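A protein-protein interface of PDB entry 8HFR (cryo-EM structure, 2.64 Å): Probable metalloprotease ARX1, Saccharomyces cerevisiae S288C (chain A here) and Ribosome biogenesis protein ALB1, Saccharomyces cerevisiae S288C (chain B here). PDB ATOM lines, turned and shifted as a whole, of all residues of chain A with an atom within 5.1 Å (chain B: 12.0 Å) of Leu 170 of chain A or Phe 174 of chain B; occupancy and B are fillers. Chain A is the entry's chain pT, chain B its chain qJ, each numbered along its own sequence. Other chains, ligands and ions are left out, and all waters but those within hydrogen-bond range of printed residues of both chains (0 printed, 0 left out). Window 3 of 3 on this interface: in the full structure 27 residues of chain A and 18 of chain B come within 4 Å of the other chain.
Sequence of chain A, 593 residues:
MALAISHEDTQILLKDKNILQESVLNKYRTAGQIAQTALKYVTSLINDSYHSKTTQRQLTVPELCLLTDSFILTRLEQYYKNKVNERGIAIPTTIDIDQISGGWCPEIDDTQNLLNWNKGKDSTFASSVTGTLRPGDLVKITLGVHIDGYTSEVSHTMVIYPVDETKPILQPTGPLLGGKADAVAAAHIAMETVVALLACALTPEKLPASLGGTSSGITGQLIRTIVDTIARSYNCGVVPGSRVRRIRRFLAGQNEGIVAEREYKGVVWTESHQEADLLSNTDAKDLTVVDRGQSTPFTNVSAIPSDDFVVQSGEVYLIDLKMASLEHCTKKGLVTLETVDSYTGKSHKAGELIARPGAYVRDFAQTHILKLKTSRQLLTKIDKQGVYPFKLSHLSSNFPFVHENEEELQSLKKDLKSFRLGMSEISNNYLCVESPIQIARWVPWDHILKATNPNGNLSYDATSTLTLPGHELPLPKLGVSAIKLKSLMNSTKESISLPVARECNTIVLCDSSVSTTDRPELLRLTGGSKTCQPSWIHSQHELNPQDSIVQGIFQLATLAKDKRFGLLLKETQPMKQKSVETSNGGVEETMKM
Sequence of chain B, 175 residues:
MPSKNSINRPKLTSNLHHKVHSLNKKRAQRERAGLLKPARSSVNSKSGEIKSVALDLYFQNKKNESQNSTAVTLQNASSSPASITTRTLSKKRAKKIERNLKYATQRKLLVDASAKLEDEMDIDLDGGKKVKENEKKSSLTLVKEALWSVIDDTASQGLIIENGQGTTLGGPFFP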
ATOM      1  N   ASN A  47     -24.815  12.396  24.561  1.00  0.00           N
ATOM      2  CA  ASN A  47     -24.688  13.830  24.313  1.00  0.00           C
ATOM      3  C   ASN A  47     -23.298  14.344  24.660  1.00  0.00           C
ATOM      4  O   ASN A  47     -22.746  15.184  23.942  1.00  0.00           O
ATOM      5  CB  ASN A  47     -25.736  14.594  25.115  1.00  0.00           C
ATOM      6  CG  ASN A  47     -27.021  14.757  24.368  1.00  0.00           C
ATOM      7  OD1 ASN A  47     -27.031  14.868  23.150  1.00  0.00           O
ATOM      8  ND2 ASN A  47     -28.123  14.767  25.094  1.00  0.00           N
ATOM      9  N   HIS A  51     -22.094  15.241  21.083  1.00  0.00           N
ATOM     10  CA  HIS A  51     -22.624  16.572  20.827  1.00  0.00           C
ATOM     11  C   HIS A  51     -21.858  17.670  21.552  1.00  0.00           C
ATOM     12  O   HIS A  51     -22.236  18.838  21.458  1.00  0.00           O
ATOM     13  CB  HIS A  51     -24.106  16.619  21.194  1.00  0.00           C
ATOM     14  CG  HIS A  51     -24.977  15.847  20.257  1.00  0.00           C
ATOM     15  ND1 HIS A  51     -26.205  15.347  20.621  1.00  0.00           N
ATOM     16  CD2 HIS A  51     -24.794  15.488  18.966  1.00  0.00           C
ATOM     17  CE1 HIS A  51     -26.743  14.711  19.595  1.00  0.00           C
ATOM     18  NE2 HIS A  51     -25.908  14.787  18.578  1.00  0.00           N
ATOM     19  N   SER A  52     -20.803  17.321  22.271  1.00  0.00           N
ATOM     20  CA  SER A  52     -19.824  18.267  22.787  1.00  0.00           C
ATOM     21  C   SER A  52     -18.431  18.004  22.247  1.00  0.00           C
ATOM     22  O   SER A  52     -17.763  18.949  21.819  1.00  0.00           O
ATOM     23  CB  SER A  52     -19.782  18.225  24.321  1.00  0.00           C
ATOM     24  OG  SER A  52     -21.044  18.515  24.887  1.00  0.00           O
ATOM     25  N   TYR A 161     -26.444  14.551  15.355  1.00  0.00           N
ATOM     26  CA  TYR A 161     -26.439  15.833  14.672  1.00  0.00           C
ATOM     27  C   TYR A 161     -25.036  16.308  14.329  1.00  0.00           C
ATOM     28  O   TYR A 161     -24.052  15.860  14.923  1.00  0.00           O
ATOM     29  CB  TYR A 161     -27.107  16.893  15.555  1.00  0.00           C
ATOM     30  CG  TYR A 161     -28.599  16.869  15.486  1.00  0.00           C
ATOM     31  CD1 TYR A 161     -29.250  17.117  14.292  1.00  0.00           C
ATOM     32  CD2 TYR A 161     -29.357  16.604  16.607  1.00  0.00           C
ATOM     33  CE1 TYR A 161     -30.619  17.095  14.218  1.00  0.00           C
ATOM     34  CE2 TYR A 161     -30.724  16.579  16.544  1.00  0.00           C
ATOM     35  CZ  TYR A 161     -31.349  16.826  15.346  1.00  0.00           C
ATOM     36  OH  TYR A 161     -32.716  16.805  15.272  1.00  0.00           O
ATOM     37  N   PRO A 162     -24.907  17.219  13.363  1.00  0.00           N
ATOM     38  CA  PRO A 162     -23.681  18.012  13.264  1.00  0.00           C
ATOM     39  C   PRO A 162     -23.771  19.212  14.192  1.00  0.00           C
ATOM     40  O   PRO A 162     -24.862  19.654  14.562  1.00  0.00           O
ATOM     41  CB  PRO A 162     -23.649  18.445  11.793  1.00  0.00           C
ATOM     42  CG  PRO A 162     -24.789  17.751  11.134  1.00  0.00           C
ATOM     43  CD  PRO A 162     -25.769  17.437  12.197  1.00  0.00           C
ATOM     44  N   VAL A 163     -22.618  19.737  14.570  1.00  0.00           N
ATOM     45  CA  VAL A 163     -22.559  20.815  15.543  1.00  0.00           C
ATOM     46  C   VAL A 163     -22.407  22.144  14.806  1.00  0.00           C
ATOM     47  O   VAL A 163     -21.996  22.195  13.646  1.00  0.00           O
ATOM     48  CB  VAL A 163     -21.408  20.564  16.545  1.00  0.00           C
ATOM     49  CG1 VAL A 163     -20.045  20.837  15.908  1.00  0.00           C
ATOM     50  CG2 VAL A 163     -21.615  21.303  17.872  1.00  0.00           C
ATOM     51  N   PRO A 168     -21.388  30.332  20.535  1.00  0.00           N
ATOM     52  CA  PRO A 168     -20.576  29.846  21.658  1.00  0.00           C
ATOM     53  C   PRO A 168     -21.196  28.649  22.344  1.00  0.00           C
ATOM     54  O   PRO A 168     -20.488  27.878  23.003  1.00  0.00           O
ATOM     55  CB  PRO A 168     -20.510  31.063  22.592  1.00  0.00           C
ATOM     56  CG  PRO A 168     -21.754  31.812  22.301  1.00  0.00           C
ATOM     57  CD  PRO A 168     -22.004  31.638  20.828  1.00  0.00           C
ATOM     58  N   ILE A 169     -22.504  28.469  22.202  1.00  0.00           N
ATOM     59  CA  ILE A 169     -23.248  27.431  22.896  1.00  0.00           C
ATOM     60  C   ILE A 169     -23.642  26.377  21.873  1.00  0.00           C
ATOM     61  O   ILE A 169     -24.038  26.710  20.750  1.00  0.00           O
ATOM     62  CB  ILE A 169     -24.480  28.025  23.602  1.00  0.00           C
ATOM     63  CG1 ILE A 169     -24.081  29.288  24.374  1.00  0.00           C
ATOM     64  CG2 ILE A 169     -25.097  27.016  24.557  1.00  0.00           C
ATOM     65  CD1 ILE A 169     -23.054  29.071  25.467  1.00  0.00           C
ATOM     66  N   LEU A 170     -23.525  25.108  22.256  1.00  0.00           N
ATOM     67  CA  LEU A 170     -23.722  24.003  21.324  1.00  0.00           C
ATOM     68  C   LEU A 170     -25.197  23.853  20.970  1.00  0.00           C
ATOM     69  O   LEU A 170     -26.049  23.713  21.852  1.00  0.00           O
ATOM     70  CB  LEU A 170     -23.175  22.713  21.926  1.00  0.00           C
ATOM     71  CG  LEU A 170     -21.729  22.818  22.418  1.00  0.00           C
ATOM     72  CD1 LEU A 170     -21.387  21.694  23.377  1.00  0.00           C
ATOM     73  CD2 LEU A 170     -20.763  22.840  21.245  1.00  0.00           C
ATOM     74  N   GLN A 171     -25.491  23.885  19.678  1.00  0.00           N
ATOM     75  CA  GLN A 171     -26.834  23.729  19.148  1.00  0.00           C
ATOM     76  C   GLN A 171     -26.740  22.990  17.823  1.00  0.00           C
ATOM     77  O   GLN A 171     -25.681  22.982  17.188  1.00  0.00           O
ATOM     78  CB  GLN A 171     -27.517  25.089  18.964  1.00  0.00           C
ATOM     79  CG  GLN A 171     -26.885  25.997  17.945  1.00  0.00           C
ATOM     80  CD  GLN A 171     -27.393  27.420  18.063  1.00  0.00           C
ATOM     81  OE1 GLN A 171     -28.405  27.680  18.713  1.00  0.00           O
ATOM     82  NE2 GLN A 171     -26.706  28.346  17.413  1.00  0.00           N
ATOM     83  N   PRO A 172     -27.811  22.310  17.407  1.00  0.00           N
ATOM     84  CA  PRO A 172     -27.816  21.687  16.080  1.00  0.00           C
ATOM     85  C   PRO A 172     -27.728  22.710  14.958  1.00  0.00           C
ATOM     86  O   PRO A 172     -28.137  23.864  15.102  1.00  0.00           O
ATOM     87  CB  PRO A 172     -29.153  20.945  16.043  1.00  0.00           C
ATOM     88  CG  PRO A 172     -29.460  20.660  17.441  1.00  0.00           C
ATOM     89  CD  PRO A 172     -28.906  21.793  18.247  1.00  0.00           C
ATOM     90  N   LEU B 169     -41.276  19.141  15.161  1.00  0.00           N
ATOM     91  CA  LEU B 169     -41.171  18.823  16.578  1.00  0.00           C
ATOM     92  C   LEU B 169     -39.754  19.118  17.037  1.00  0.00           C
ATOM     93  O   LEU B 169     -38.805  19.036  16.255  1.00  0.00           O
ATOM     94  CB  LEU B 169     -41.504  17.353  16.885  1.00  0.00           C
ATOM     95  CG  LEU B 169     -42.732  16.668  16.279  1.00  0.00           C
ATOM     96  CD1 LEU B 169     -42.589  15.159  16.357  1.00  0.00           C
ATOM     97  CD2 LEU B 169     -44.004  17.117  16.961  1.00  0.00           C
ATOM     98  N   GLY B 170     -39.618  19.477  18.312  1.00  0.00           N
ATOM     99  CA  GLY B 170     -38.317  19.775  18.880  1.00  0.00           C
ATOM    100  C   GLY B 170     -37.754  21.117  18.464  1.00  0.00           C
ATOM    101  O   GLY B 170     -38.260  21.752  17.537  1.00  0.00           O
ATOM    102  N   GLY B 171     -36.703  21.567  19.138  1.00  0.00           N
ATOM    103  CA  GLY B 171     -36.157  22.876  18.881  1.00  0.00           C
ATOM    104  C   GLY B 171     -34.661  22.860  18.662  1.00  0.00           C
ATOM    105  O   GLY B 171     -34.041  21.801  18.537  1.00  0.00           O
ATOM    106  N   PRO B 172     -34.040  24.046  18.641  1.00  0.00           N
ATOM    107  CA  PRO B 172     -32.594  24.125  18.384  1.00  0.00           C
ATOM    108  C   PRO B 172     -31.736  23.870  19.613  1.00  0.00           C
ATOM    109  O   PRO B 172     -30.569  24.256  19.652  1.00  0.00           O
ATOM    110  CB  PRO B 172     -32.420  25.554  17.870  1.00  0.00           C
ATOM    111  CG  PRO B 172     -33.494  26.309  18.552  1.00  0.00           C
ATOM    112  CD  PRO B 172     -34.665  25.379  18.664  1.00  0.00           C
ATOM    113  N   PHE B 173     -32.317  23.260  20.632  1.00  0.00           N
ATOM    114  CA  PHE B 173     -31.626  22.792  21.821  1.00  0.00           C
ATOM    115  C   PHE B 173     -31.354  21.296  21.701  1.00  0.00           C
ATOM    116  O   PHE B 173     -32.027  20.590  20.949  1.00  0.00           O
ATOM    117  CB  PHE B 173     -32.468  23.076  23.067  1.00  0.00           C
ATOM    118  CG  PHE B 173     -33.642  22.143  23.245  1.00  0.00           C
ATOM    119  CD1 PHE B 173     -34.726  22.172  22.372  1.00  0.00           C
ATOM    120  CD2 PHE B 173     -33.673  21.251  24.299  1.00  0.00           C
ATOM    121  CE1 PHE B 173     -35.795  21.318  22.534  1.00  0.00           C
ATOM    122  CE2 PHE B 173     -34.745  20.395  24.470  1.00  0.00           C
ATOM    123  CZ  PHE B 173     -35.806  20.430  23.585  1.00  0.00           C
ATOM    124  N   PHE B 174     -30.351  20.815  22.438  1.00  0.00           N
ATOM    125  CA  PHE B 174     -30.085  19.382  22.512  1.00  0.00           C
ATOM    126  C   PHE B 174     -30.958  18.779  23.598  1.00  0.00           C
ATOM    127  O   PHE B 174     -30.777  19.117  24.778  1.00  0.00           O
ATOM    128  CB  PHE B 174     -28.619  19.101  22.805  1.00  0.00           C
ATOM    129  CG  PHE B 174     -27.743  19.125  21.593  1.00  0.00           C
ATOM    130  CD1 PHE B 174     -28.004  18.290  20.524  1.00  0.00           C
ATOM    131  CD2 PHE B 174     -26.647  19.964  21.531  1.00  0.00           C
ATOM    132  CE1 PHE B 174     -27.204  18.311  19.410  1.00  0.00           C
ATOM    133  CE2 PHE B 174     -25.841  19.982  20.421  1.00  0.00           C
ATOM    134  CZ  PHE B 174     -26.121  19.157  19.359  1.00  0.00           C
ATOM    135  N   PRO B 175     -31.902  17.887  23.267  1.00  0.00           N
ATOM    136  CA  PRO B 175     -32.760  17.271  24.277  1.00  0.00           C
ATOM    137  C   PRO B 175     -32.070  16.106  24.977  1.00  0.00           C
ATOM    138  O   PRO B 175     -31.099  15.578  24.434  1.00  0.00           O
ATOM    139  CB  PRO B 175     -33.957  16.792  23.462  1.00  0.00           C
ATOM    140  CG  PRO B 175     -33.380  16.464  22.144  1.00  0.00           C
ATOM    141  CD  PRO B 175     -32.235  17.417  21.912  1.00  0.00           C
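Among the printed residues, 8 pairs touch across the chains.
Among the printed residues, pairs that only touch across the chains: His 51 of chain A with Phe 174 of chain B (3.4 Å), Tyr 161 of chain A with Phe 174 of chain B (3.9 Å), Leu 170 of chain A with Phe 174 of chain B (3.8 Å), Gln 171 of chain A with Pro 172 of chain B (3.2 Å), Gln 171 of chain A with Phe 174 of chain B (3.99 Å), Pro 172 of chain A with Pro 172 of chain B (3.3 Å) and Pro 172 of chain A with Phe 174 of chain B (3.8 Å).
A ring nitrogen (ND1) of His 51 of chain A is in hydrogen-bond range of the side-chain amide oxygen (OD1) of Asn 47 of chain A (2.7 Å).
The backbone carbonyl oxygen (O) of Asn 47 of chain A lies within hydrogen-bond range of the backbone NH (N) of Ser 52 of chain A (3.3 Å).
NE2 of His 51 of chain A lies within hydrogen-bond range of N of Tyr 161 of chain A.
Of chain B, only Phe 174 comes within 4 Å of Leu 170 of chain A.
Of the printed residues of chain A, Phe 174 of chain B touches His 51 (3.4 Å), Tyr 161 (3.9 Å), Leu 170 (3.8 Å), Gln 171 (3.99 Å) and Pro 172 (3.8 Å).
Of chain B, only Phe 174 (3.4 Å) comes within 4 Å of His 51 of chain A.
No residue of chain B comes within 4 Å of Val 163 of chain A.
No residue of chain B comes within 4 Å of Pro 168 of chain A.
Ile 169 of chain A touches none of the printed residues of chain B.
Pro 172 of chain A touches two residues of chain B.
Printed residues of chain A within 4 Å of Pro 175 of chain B: Asn 47 (3.2 Å).
Of the printed residues of chain B, Gln 171 of chain A touches Pro 172 and Phe 174.
Printed residues of chain A within 4 Å of Pro 172 of chain B: Gln 171 and Pro 172.
Pro 162 of chain A touches none of the printed residues of chain B.
Gly 170 of chain B touches none of the printed residues of chain A.
The nearest printed residue of chain A that does not touch Pro 175 of chain B is Tyr 161 of chain A (5.6 Å).
ND2 of Asn 47 of chain A lies within hydrogen-bond range of O of Pro 175 of chain B (3.2 Å).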
